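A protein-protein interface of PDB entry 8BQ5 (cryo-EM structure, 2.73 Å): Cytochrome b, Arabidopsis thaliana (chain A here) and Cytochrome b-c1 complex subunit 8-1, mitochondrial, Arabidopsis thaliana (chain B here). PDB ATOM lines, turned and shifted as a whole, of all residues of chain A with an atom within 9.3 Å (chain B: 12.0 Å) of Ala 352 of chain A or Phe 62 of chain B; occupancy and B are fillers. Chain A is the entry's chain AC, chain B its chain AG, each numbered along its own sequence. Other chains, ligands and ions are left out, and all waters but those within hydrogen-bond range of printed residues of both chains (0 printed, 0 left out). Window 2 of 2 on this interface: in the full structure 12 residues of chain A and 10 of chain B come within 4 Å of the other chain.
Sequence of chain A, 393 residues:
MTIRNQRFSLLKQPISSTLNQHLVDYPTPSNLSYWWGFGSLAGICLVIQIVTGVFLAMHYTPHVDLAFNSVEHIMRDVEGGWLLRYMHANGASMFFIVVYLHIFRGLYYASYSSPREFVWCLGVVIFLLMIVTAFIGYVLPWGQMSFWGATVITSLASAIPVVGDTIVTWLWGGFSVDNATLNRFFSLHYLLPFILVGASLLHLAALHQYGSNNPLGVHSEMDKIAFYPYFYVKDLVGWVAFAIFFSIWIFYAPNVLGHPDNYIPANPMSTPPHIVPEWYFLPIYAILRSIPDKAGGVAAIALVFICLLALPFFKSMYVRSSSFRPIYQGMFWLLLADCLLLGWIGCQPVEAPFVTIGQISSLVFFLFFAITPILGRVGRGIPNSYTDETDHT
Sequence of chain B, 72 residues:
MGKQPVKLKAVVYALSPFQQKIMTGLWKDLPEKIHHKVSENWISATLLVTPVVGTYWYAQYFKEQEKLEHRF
Hydrophobic or aromatic side chains of chain B within 4 Å of the printed part of chain A: Tyr 56, Ala 59 and Phe 62. Among the printed residues, 6 pairs touch across the chains.
The backbone carbonyl oxygen (O) of Tyr 56 of chain B lies close to the side-chain amide nitrogen (NE2) of Gln 60 of chain B, 3.2 Å away. O of Trp 344 of chain A lies close to NE2 of Gln 348 of chain A (3.3 Å).
Among the printed residues, pairs that only touch across the chains: Pro 353 of chain A with Phe 62 of chain B, Trp 344 of chain A with Ala 59 of chain B, Trp 344 of chain A with Tyr 56 of chain B, Ile 357 of chain A with Thr 55 of chain B, Ala 352 of chain A with Phe 62 of chain B and Phe 354 of chain A with Ala 59 of chain B.
Of the printed residues of chain B, Trp 344 of chain A touches Tyr 56 (3.7 Å) and Ala 59 (3.6 Å). Ile 345 of chain A touches none of the printed residues of chain B. Printed residues of chain B within 4 Å of Ala 352 of chain A: Phe 62. Of chain B, only Phe 62 comes within 4 Å of Pro 353 of chain A. Val 355 of chain A touches none of the printed residues of chain B. Of the printed residues of chain B, Ile 357 of chain A touches Thr 55 (3.8 Å). Phe 62 of chain B touches just these residues of chain A: Ala 352 (3.9 Å) and Pro 353 (3.5 Å). Arg 71 of chain B touches none of the printed residues of chain A. The nearest residue of chain B that does not touch Ala 352 of chain A is Glu 66 of chain B (5.5 Å).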
ATOM      1  N   TRP A 344       1.669  -4.857  23.198  1.00  0.00           N
ATOM      2  CA  TRP A 344       2.069  -3.455  23.191  1.00  0.00           C
ATOM      3  C   TRP A 344       3.583  -3.314  23.292  1.00  0.00           C
ATOM      4  O   TRP A 344       4.175  -2.432  22.661  1.00  0.00           O
ATOM      5  CB  TRP A 344       1.372  -2.716  24.334  1.00  0.00           C
ATOM      6  CG  TRP A 344       1.881  -1.333  24.586  1.00  0.00           C
ATOM      7  CD1 TRP A 344       1.689  -0.233  23.805  1.00  0.00           C
ATOM      8  CD2 TRP A 344       2.648  -0.894  25.713  1.00  0.00           C
ATOM      9  NE1 TRP A 344       2.299   0.860  24.367  1.00  0.00           N
ATOM     10  CE2 TRP A 344       2.894   0.481  25.541  1.00  0.00           C
ATOM     11  CE3 TRP A 344       3.156  -1.532  26.849  1.00  0.00           C
ATOM     12  CZ2 TRP A 344       3.625   1.230  26.460  1.00  0.00           C
ATOM     13  CZ3 TRP A 344       3.880  -0.787  27.761  1.00  0.00           C
ATOM     14  CH2 TRP A 344       4.108   0.580  27.561  1.00  0.00           C
ATOM     15  N   ILE A 345       4.223  -4.180  24.079  1.00  0.00           N
ATOM     16  CA  ILE A 345       5.675  -4.130  24.232  1.00  0.00           C
ATOM     17  C   ILE A 345       6.368  -4.471  22.918  1.00  0.00           C
ATOM     18  O   ILE A 345       7.389  -3.869  22.565  1.00  0.00           O
ATOM     19  CB  ILE A 345       6.118  -5.063  25.374  1.00  0.00           C
ATOM     20  CG1 ILE A 345       5.822  -4.417  26.728  1.00  0.00           C
ATOM     21  CG2 ILE A 345       7.592  -5.411  25.256  1.00  0.00           C
ATOM     22  CD1 ILE A 345       6.733  -3.255  27.052  1.00  0.00           C
ATOM     23  N   GLN A 348       7.101  -1.615  20.626  1.00  0.00           N
ATOM     24  CA  GLN A 348       8.056  -0.663  21.167  1.00  0.00           C
ATOM     25  C   GLN A 348       9.479  -1.031  20.766  1.00  0.00           C
ATOM     26  O   GLN A 348       9.795  -2.211  20.582  1.00  0.00           O
ATOM     27  CB  GLN A 348       7.963  -0.618  22.695  1.00  0.00           C
ATOM     28  CG  GLN A 348       6.566  -0.384  23.225  1.00  0.00           C
ATOM     29  CD  GLN A 348       5.953   0.893  22.699  1.00  0.00           C
ATOM     30  OE1 GLN A 348       6.522   1.973  22.842  1.00  0.00           O
ATOM     31  NE2 GLN A 348       4.782   0.777  22.087  1.00  0.00           N
ATOM     32  N   PRO A 349      10.364  -0.045  20.632  1.00  0.00           N
ATOM     33  CA  PRO A 349      11.766  -0.356  20.336  1.00  0.00           C
ATOM     34  C   PRO A 349      12.456  -0.970  21.542  1.00  0.00           C
ATOM     35  O   PRO A 349      12.043  -0.784  22.688  1.00  0.00           O
ATOM     36  CB  PRO A 349      12.372   1.009  19.978  1.00  0.00           C
ATOM     37  CG  PRO A 349      11.215   1.986  19.958  1.00  0.00           C
ATOM     38  CD  PRO A 349      10.157   1.397  20.822  1.00  0.00           C
ATOM     39  N   VAL A 350      13.530  -1.708  21.268  1.00  0.00           N
ATOM     40  CA  VAL A 350      14.231  -2.446  22.310  1.00  0.00           C
ATOM     41  C   VAL A 350      15.140  -1.500  23.082  1.00  0.00           C
ATOM     42  O   VAL A 350      16.296  -1.280  22.706  1.00  0.00           O
ATOM     43  CB  VAL A 350      15.031  -3.620  21.719  1.00  0.00           C
ATOM     44  CG1 VAL A 350      15.588  -4.495  22.831  1.00  0.00           C
ATOM     45  CG2 VAL A 350      14.157  -4.432  20.780  1.00  0.00           C
ATOM     46  N   GLU A 351      14.616  -0.938  24.169  1.00  0.00           N
ATOM     47  CA  GLU A 351      15.363  -0.022  25.018  1.00  0.00           C
ATOM     48  C   GLU A 351      14.599   0.136  26.324  1.00  0.00           C
ATOM     49  O   GLU A 351      13.467  -0.330  26.462  1.00  0.00           O
ATOM     50  CB  GLU A 351      15.578   1.330  24.332  1.00  0.00           C
ATOM     51  CG  GLU A 351      14.352   2.219  24.333  1.00  0.00           C
ATOM     52  CD  GLU A 351      14.194   2.988  23.040  1.00  0.00           C
ATOM     53  OE1 GLU A 351      15.148   3.687  22.641  1.00  0.00           O
ATOM     54  OE2 GLU A 351      13.111   2.900  22.428  1.00  0.00           O
ATOM     55  N   ALA A 352      15.235   0.801  27.283  1.00  0.00           N
ATOM     56  CA  ALA A 352      14.611   0.997  28.583  1.00  0.00           C
ATOM     57  C   ALA A 352      13.376   1.886  28.447  1.00  0.00           C
ATOM     58  O   ALA A 352      13.356   2.800  27.617  1.00  0.00           O
ATOM     59  CB  ALA A 352      15.601   1.621  29.565  1.00  0.00           C
ATOM     60  N   PRO A 353      12.326   1.643  29.243  1.00  0.00           N
ATOM     61  CA  PRO A 353      12.179   0.603  30.265  1.00  0.00           C
ATOM     62  C   PRO A 353      11.549  -0.662  29.704  1.00  0.00           C
ATOM     63  O   PRO A 353      11.181  -1.567  30.445  1.00  0.00           O
ATOM     64  CB  PRO A 353      11.268   1.279  31.294  1.00  0.00           C
ATOM     65  CG  PRO A 353      10.439   2.288  30.487  1.00  0.00           C
ATOM     66  CD  PRO A 353      11.085   2.424  29.119  1.00  0.00           C
ATOM     67  N   PHE A 354      11.405  -0.739  28.381  1.00  0.00           N
ATOM     68  CA  PHE A 354      10.656  -1.823  27.761  1.00  0.00           C
ATOM     69  C   PHE A 354      11.368  -3.164  27.846  1.00  0.00           C
ATOM     70  O   PHE A 354      10.712  -4.205  27.729  1.00  0.00           O
ATOM     71  CB  PHE A 354      10.365  -1.473  26.303  1.00  0.00           C
ATOM     72  CG  PHE A 354       9.626  -0.180  26.138  1.00  0.00           C
ATOM     73  CD1 PHE A 354       8.377  -0.004  26.707  1.00  0.00           C
ATOM     74  CD2 PHE A 354      10.187   0.868  25.429  1.00  0.00           C
ATOM     75  CE1 PHE A 354       7.696   1.185  26.560  1.00  0.00           C
ATOM     76  CE2 PHE A 354       9.511   2.061  25.280  1.00  0.00           C
ATOM     77  CZ  PHE A 354       8.264   2.220  25.847  1.00  0.00           C
ATOM     78  N   VAL A 355      12.686  -3.170  28.044  1.00  0.00           N
ATOM     79  CA  VAL A 355      13.396  -4.431  28.230  1.00  0.00           C
ATOM     80  C   VAL A 355      13.006  -5.066  29.560  1.00  0.00           C
ATOM     81  O   VAL A 355      12.702  -6.261  29.628  1.00  0.00           O
ATOM     82  CB  VAL A 355      14.915  -4.211  28.129  1.00  0.00           C
ATOM     83  CG1 VAL A 355      15.647  -5.531  28.249  1.00  0.00           C
ATOM     84  CG2 VAL A 355      15.257  -3.536  26.814  1.00  0.00           C
ATOM     85  N   THR A 356      13.002  -4.273  30.635  1.00  0.00           N
ATOM     86  CA  THR A 356      12.613  -4.801  31.939  1.00  0.00           C
ATOM     87  C   THR A 356      11.140  -5.189  31.961  1.00  0.00           C
ATOM     88  O   THR A 356      10.770  -6.222  32.530  1.00  0.00           O
ATOM     89  CB  THR A 356      12.909  -3.777  33.034  1.00  0.00           C
ATOM     90  OG1 THR A 356      14.287  -3.389  32.968  1.00  0.00           O
ATOM     91  CG2 THR A 356      12.625  -4.367  34.406  1.00  0.00           C
ATOM     92  N   ILE A 357      10.283  -4.369  31.348  1.00  0.00           N
ATOM     93  CA  ILE A 357       8.853  -4.662  31.331  1.00  0.00           C
ATOM     94  C   ILE A 357       8.579  -5.941  30.550  1.00  0.00           C
ATOM     95  O   ILE A 357       7.770  -6.779  30.965  1.00  0.00           O
ATOM     96  CB  ILE A 357       8.069  -3.468  30.758  1.00  0.00           C
ATOM     97  CG1 ILE A 357       8.229  -2.247  31.663  1.00  0.00           C
ATOM     98  CG2 ILE A 357       6.599  -3.817  30.609  1.00  0.00           C
ATOM     99  CD1 ILE A 357       7.754  -0.962  31.033  1.00  0.00           C
ATOM    100  N   GLY A 358       9.243  -6.107  29.405  1.00  0.00           N
ATOM    101  CA  GLY A 358       9.037  -7.308  28.610  1.00  0.00           C
ATOM    102  C   GLY A 358       9.509  -8.566  29.313  1.00  0.00           C
ATOM    103  O   GLY A 358       8.892  -9.626  29.187  1.00  0.00           O
ATOM    104  N   VAL B  53      -3.066  -0.094  32.566  1.00  0.00           N
ATOM    105  CA  VAL B  53      -2.968   1.352  32.746  1.00  0.00           C
ATOM    106  C   VAL B  53      -1.750   1.707  33.589  1.00  0.00           C
ATOM    107  O   VAL B  53      -1.039   2.676  33.298  1.00  0.00           O
ATOM    108  CB  VAL B  53      -4.269   1.899  33.357  1.00  0.00           C
ATOM    109  CG1 VAL B  53      -4.115   3.369  33.726  1.00  0.00           C
ATOM    110  CG2 VAL B  53      -5.416   1.714  32.383  1.00  0.00           C
ATOM    111  N   GLY B  54      -1.489   0.931  34.643  1.00  0.00           N
ATOM    112  CA  GLY B  54      -0.331   1.204  35.478  1.00  0.00           C
ATOM    113  C   GLY B  54       0.977   1.059  34.726  1.00  0.00           C
ATOM    114  O   GLY B  54       1.896   1.865  34.891  1.00  0.00           O
ATOM    115  N   THR B  55       1.081   0.026  33.889  1.00  0.00           N
ATOM    116  CA  THR B  55       2.297  -0.164  33.106  1.00  0.00           C
ATOM    117  C   THR B  55       2.429   0.901  32.025  1.00  0.00           C
ATOM    118  O   THR B  55       3.526   1.418  31.787  1.00  0.00           O
ATOM    119  CB  THR B  55       2.312  -1.561  32.486  1.00  0.00           C
ATOM    120  OG1 THR B  55       2.117  -2.540  33.514  1.00  0.00           O
ATOM    121  CG2 THR B  55       3.640  -1.824  31.801  1.00  0.00           C
ATOM    122  N   TYR B  56       1.322   1.241  31.362  1.00  0.00           N
ATOM    123  CA  TYR B  56       1.363   2.271  30.329  1.00  0.00           C
ATOM    124  C   TYR B  56       1.754   3.621  30.915  1.00  0.00           C
ATOM    125  O   TYR B  56       2.589   4.335  30.350  1.00  0.00           O
ATOM    126  CB  TYR B  56       0.010   2.363  29.624  1.00  0.00           C
ATOM    127  CG  TYR B  56      -0.004   3.313  28.445  1.00  0.00           C
ATOM    128  CD1 TYR B  56       0.369   2.883  27.180  1.00  0.00           C
ATOM    129  CD2 TYR B  56      -0.391   4.637  28.600  1.00  0.00           C
ATOM    130  CE1 TYR B  56       0.356   3.745  26.102  1.00  0.00           C
ATOM    131  CE2 TYR B  56      -0.406   5.506  27.528  1.00  0.00           C
ATOM    132  CZ  TYR B  56      -0.032   5.055  26.282  1.00  0.00           C
ATOM    133  OH  TYR B  56      -0.047   5.918  25.211  1.00  0.00           O
ATOM    134  N   TRP B  57       1.162   3.988  32.055  1.00  0.00           N
ATOM    135  CA  TRP B  57       1.494   5.269  32.670  1.00  0.00           C
ATOM    136  C   TRP B  57       2.952   5.313  33.106  1.00  0.00           C
ATOM    137  O   TRP B  57       3.622   6.340  32.950  1.00  0.00           O
ATOM    138  CB  TRP B  57       0.577   5.552  33.862  1.00  0.00           C
ATOM    139  CG  TRP B  57       1.202   6.497  34.848  1.00  0.00           C
ATOM    140  CD1 TRP B  57       1.134   7.861  34.831  1.00  0.00           C
ATOM    141  CD2 TRP B  57       1.995   6.151  35.992  1.00  0.00           C
ATOM    142  NE1 TRP B  57       1.838   8.383  35.889  1.00  0.00           N
ATOM    143  CE2 TRP B  57       2.377   7.355  36.616  1.00  0.00           C
ATOM    144  CE3 TRP B  57       2.422   4.940  36.547  1.00  0.00           C
ATOM    145  CZ2 TRP B  57       3.162   7.382  37.766  1.00  0.00           C
ATOM    146  CZ3 TRP B  57       3.204   4.970  37.687  1.00  0.00           C
ATOM    147  CH2 TRP B  57       3.565   6.183  38.285  1.00  0.00           C
ATOM    148  N   TYR B  58       3.458   4.214  33.669  1.00  0.00           N
ATOM    149  CA  TYR B  58       4.840   4.203  34.136  1.00  0.00           C
ATOM    150  C   TYR B  58       5.816   4.371  32.979  1.00  0.00           C
ATOM    151  O   TYR B  58       6.837   5.053  33.114  1.00  0.00           O
ATOM    152  CB  TYR B  58       5.134   2.912  34.899  1.00  0.00           C
ATOM    153  CG  TYR B  58       6.597   2.743  35.235  1.00  0.00           C
ATOM    154  CD1 TYR B  58       7.372   1.790  34.590  1.00  0.00           C
ATOM    155  CD2 TYR B  58       7.206   3.545  36.190  1.00  0.00           C
ATOM    156  CE1 TYR B  58       8.710   1.636  34.889  1.00  0.00           C
ATOM    157  CE2 TYR B  58       8.546   3.398  36.497  1.00  0.00           C
ATOM    158  CZ  TYR B  58       9.291   2.442  35.843  1.00  0.00           C
ATOM    159  OH  TYR B  58      10.625   2.289  36.144  1.00  0.00           O
ATOM    160  N   ALA B  59       5.520   3.749  31.835  1.00  0.00           N
ATOM    161  CA  ALA B  59       6.392   3.886  30.674  1.00  0.00           C
ATOM    162  C   ALA B  59       6.437   5.326  30.178  1.00  0.00           C
ATOM    163  O   ALA B  59       7.507   5.832  29.822  1.00  0.00           O
ATOM    164  CB  ALA B  59       5.934   2.946  29.559  1.00  0.00           C
ATOM    165  N   GLN B  60       5.286   6.004  30.138  1.00  0.00           N
ATOM    166  CA  GLN B  60       5.281   7.404  29.724  1.00  0.00           C
ATOM    167  C   GLN B  60       5.994   8.281  30.743  1.00  0.00           C
ATOM    168  O   GLN B  60       6.638   9.271  30.380  1.00  0.00           O
ATOM    169  CB  GLN B  60       3.853   7.903  29.503  1.00  0.00           C
ATOM    170  CG  GLN B  60       2.940   6.952  28.750  1.00  0.00           C
ATOM    171  CD  GLN B  60       3.584   6.370  27.509  1.00  0.00           C
ATOM    172  OE1 GLN B  60       3.813   7.072  26.524  1.00  0.00           O
ATOM    173  NE2 GLN B  60       3.872   5.076  27.547  1.00  0.00           N
ATOM    174  N   TYR B  61       5.877   7.946  32.029  1.00  0.00           N
ATOM    175  CA  TYR B  61       6.600   8.699  33.048  1.00  0.00           C
ATOM    176  C   TYR B  61       8.102   8.484  32.917  1.00  0.00           C
ATOM    177  O   TYR B  61       8.892   9.418  33.083  1.00  0.00           O
ATOM    178  CB  TYR B  61       6.113   8.303  34.441  1.00  0.00           C
ATOM    179  CG  TYR B  61       6.944   8.884  35.561  1.00  0.00           C
ATOM    180  CD1 TYR B  61       8.046   8.205  36.064  1.00  0.00           C
ATOM    181  CD2 TYR B  61       6.635  10.123  36.104  1.00  0.00           C
ATOM    182  CE1 TYR B  61       8.810   8.739  37.080  1.00  0.00           C
ATOM    183  CE2 TYR B  61       7.393  10.665  37.121  1.00  0.00           C
ATOM    184  CZ  TYR B  61       8.479   9.968  37.605  1.00  0.00           C
ATOM    185  OH  TYR B  61       9.237  10.504  38.619  1.00  0.00           O
ATOM    186  N   PHE B  62       8.516   7.244  32.639  1.00  0.00           N
ATOM    187  CA  PHE B  62       9.936   6.954  32.473  1.00  0.00           C
ATOM    188  C   PHE B  62      10.513   7.696  31.276  1.00  0.00           C
ATOM    189  O   PHE B  62      11.588   8.299  31.367  1.00  0.00           O
ATOM    190  CB  PHE B  62      10.139   5.446  32.323  1.00  0.00           C
ATOM    191  CG  PHE B  62      11.583   5.014  32.292  1.00  0.00           C
ATOM    192  CD1 PHE B  62      12.330   5.108  31.127  1.00  0.00           C
ATOM    193  CD2 PHE B  62      12.183   4.487  33.423  1.00  0.00           C
ATOM    194  CE1 PHE B  62      13.649   4.703  31.095  1.00  0.00           C
ATOM    195  CE2 PHE B  62      13.503   4.079  33.396  1.00  0.00           C
ATOM    196  CZ  PHE B  62      14.237   4.188  32.231  1.00  0.00           C
ATOM    197  N   LYS B  63       9.809   7.667  30.143  1.00  0.00           N
ATOM    198  CA  LYS B  63      10.337   8.282  28.932  1.00  0.00           C
ATOM    199  C   LYS B  63      10.361   9.801  29.046  1.00  0.00           C
ATOM    200  O   LYS B  63      11.202  10.463  28.428  1.00  0.00           O
ATOM    201  CB  LYS B  63       9.516   7.839  27.719  1.00  0.00           C
ATOM    202  CG  LYS B  63       8.478   8.849  27.270  1.00  0.00           C
ATOM    203  CD  LYS B  63       7.318   8.186  26.559  1.00  0.00           C
ATOM    204  CE  LYS B  63       6.210   9.190  26.296  1.00  0.00           C
ATOM    205  NZ  LYS B  63       5.744   9.829  27.557  1.00  0.00           N
ATOM    206  N   GLU B  64       9.450  10.375  29.835  1.00  0.00           N
ATOM    207  CA  GLU B  64       9.412  11.827  29.971  1.00  0.00           C
ATOM    208  C   GLU B  64      10.558  12.325  30.842  1.00  0.00           C
ATOM    209  O   GLU B  64      11.172  13.357  30.549  1.00  0.00           O
ATOM    210  CB  GLU B  64       8.064  12.271  30.539  1.00  0.00           C
ATOM    211  CG  GLU B  64       7.353  13.293  29.668  1.00  0.00           C
ATOM    212  CD  GLU B  64       7.991  14.667  29.742  1.00  0.00           C
ATOM    213  OE1 GLU B  64       7.754  15.484  28.828  1.00  0.00           O
ATOM    214  OE2 GLU B  64       8.722  14.934  30.716  1.00  0.00           O
ATOM    215  N   GLN B  65      10.859  11.603  31.923  1.00  0.00           N
ATOM    216  CA  GLN B  65      12.003  11.970  32.750  1.00  0.00           C
ATOM    217  C   GLN B  65      13.316  11.680  32.034  1.00  0.00           C
ATOM    218  O   GLN B  65      14.279  12.444  32.163  1.00  0.00           O
ATOM    219  CB  GLN B  65      11.948  11.233  34.089  1.00  0.00           C
ATOM    220  CG  GLN B  65      10.649  11.416  34.853  1.00  0.00           C
ATOM    221  CD  GLN B  65      10.174  12.857  34.881  1.00  0.00           C
ATOM    222  OE1 GLN B  65      10.925  13.767  35.235  1.00  0.00           O
ATOM    223  NE2 GLN B  65       8.918  13.071  34.510  1.00  0.00           N
ATOM    224  N   GLU B  66      13.377  10.578  31.282  1.00  0.00           N
ATOM    225  CA  GLU B  66      14.586  10.265  30.527  1.00  0.00           C
ATOM    226  C   GLU B  66      14.854  11.312  29.454  1.00  0.00           C
ATOM    227  O   GLU B  66      16.002  11.723  29.250  1.00  0.00           O
ATOM    228  CB  GLU B  66      14.468   8.875  29.900  1.00  0.00           C
ATOM    229  CG  GLU B  66      15.799   8.236  29.536  1.00  0.00           C
ATOM    230  CD  GLU B  66      16.603   7.813  30.751  1.00  0.00           C
ATOM    231  OE1 GLU B  66      17.599   8.494  31.071  1.00  0.00           O
ATOM    232  OE2 GLU B  66      16.244   6.798  31.383  1.00  0.00           O
ATOM    233  N   LYS B  67      13.805  11.755  28.760  1.00  0.00           N
ATOM    234  CA  LYS B  67      13.972  12.770  27.725  1.00  0.00           C
ATOM    235  C   LYS B  67      14.454  14.087  28.321  1.00  0.00           C
ATOM    236  O   LYS B  67      15.251  14.803  27.705  1.00  0.00           O
ATOM    237  CB  LYS B  67      12.655  12.959  26.971  1.00  0.00           C
ATOM    238  CG  LYS B  67      12.417  14.360  26.440  1.00  0.00           C
ATOM    239  CD  LYS B  67      11.555  14.328  25.191  1.00  0.00           C
ATOM    240  CE  LYS B  67      10.082  14.242  25.546  1.00  0.00           C
ATOM    241  NZ  LYS B  67       9.573  15.530  26.090  1.00  0.00           N
ATOM    242  N   LEU B  68      13.986  14.417  29.526  1.00  0.00           N
ATOM    243  CA  LEU B  68      14.439  15.631  30.194  1.00  0.00           C
ATOM    244  C   LEU B  68      15.885  15.516  30.662  1.00  0.00           C
ATOM    245  O   LEU B  68      16.617  16.511  30.651  1.00  0.00           O
ATOM    246  CB  LEU B  68      13.528  15.949  31.379  1.00  0.00           C
ATOM    247  CG  LEU B  68      12.133  16.481  31.058  1.00  0.00           C
ATOM    248  CD1 LEU B  68      11.222  16.310  32.261  1.00  0.00           C
ATOM    249  CD2 LEU B  68      12.198  17.939  30.630  1.00  0.00           C
ATOM    250  N   GLU B  69      16.309  14.322  31.085  1.00  0.00           N
ATOM    251  CA  GLU B  69      17.663  14.157  31.606  1.00  0.00           C
ATOM    252  C   GLU B  69      18.717  14.330  30.519  1.00  0.00           C
ATOM    253  O   GLU B  69      19.846  14.737  30.814  1.00  0.00           O
ATOM    254  CB  GLU B  69      17.814  12.786  32.268  1.00  0.00           C
ATOM    255  CG  GLU B  69      17.117  12.659  33.614  1.00  0.00           C
ATOM    256  CD  GLU B  69      18.036  12.143  34.707  1.00  0.00           C
ATOM    257  OE1 GLU B  69      19.198  11.803  34.402  1.00  0.00           O
ATOM    258  OE2 GLU B  69      17.593  12.077  35.873  1.00  0.00           O
ATOM    259  N   HIS B  70      18.377  14.028  29.270  1.00  0.00           N
ATOM    260  CA  HIS B  70      19.320  14.135  28.166  1.00  0.00           C
ATOM    261  C   HIS B  70      19.296  15.504  27.499  1.00  0.00           C
ATOM    262  O   HIS B  70      19.963  15.691  26.477  1.00  0.00           O
ATOM    263  CB  HIS B  70      19.036  13.048  27.125  1.00  0.00           C
ATOM    264  CG  HIS B  70      19.321  11.660  27.608  1.00  0.00           C
ATOM    265  ND1 HIS B  70      19.969  11.406  28.799  1.00  0.00           N
ATOM    266  CD2 HIS B  70      19.040  10.452  27.067  1.00  0.00           C
ATOM    267  CE1 HIS B  70      20.077  10.100  28.967  1.00  0.00           C
ATOM    268  NE2 HIS B  70      19.522   9.498  27.931  1.00  0.00           N
ATOM    269  N   ARG B  71      18.550  16.458  28.048  1.00  0.00           N
ATOM    270  CA  ARG B  71      18.444  17.792  27.478  1.00  0.00           C
ATOM    271  C   ARG B  71      19.448  18.723  28.146  1.00  0.00           C
ATOM    272  O   ARG B  71      19.540  18.767  29.378  1.00  0.00           O
ATOM    273  CB  ARG B  71      17.028  18.341  27.649  1.00  0.00           C
ATOM    274  CG  ARG B  71      16.158  18.213  26.416  1.00  0.00           C
ATOM    275  CD  ARG B  71      14.777  18.788  26.670  1.00  0.00           C
ATOM    276  NE  ARG B  71      13.776  18.224  25.775  1.00  0.00           N
ATOM    277  CZ  ARG B  71      12.523  18.647  25.694  1.00  0.00           C
ATOM    278  NH1 ARG B  71      12.082  19.644  26.443  1.00  0.00           N
ATOM    279  NH2 ARG B  71      11.693  18.058  24.839  1.00  0.00           N
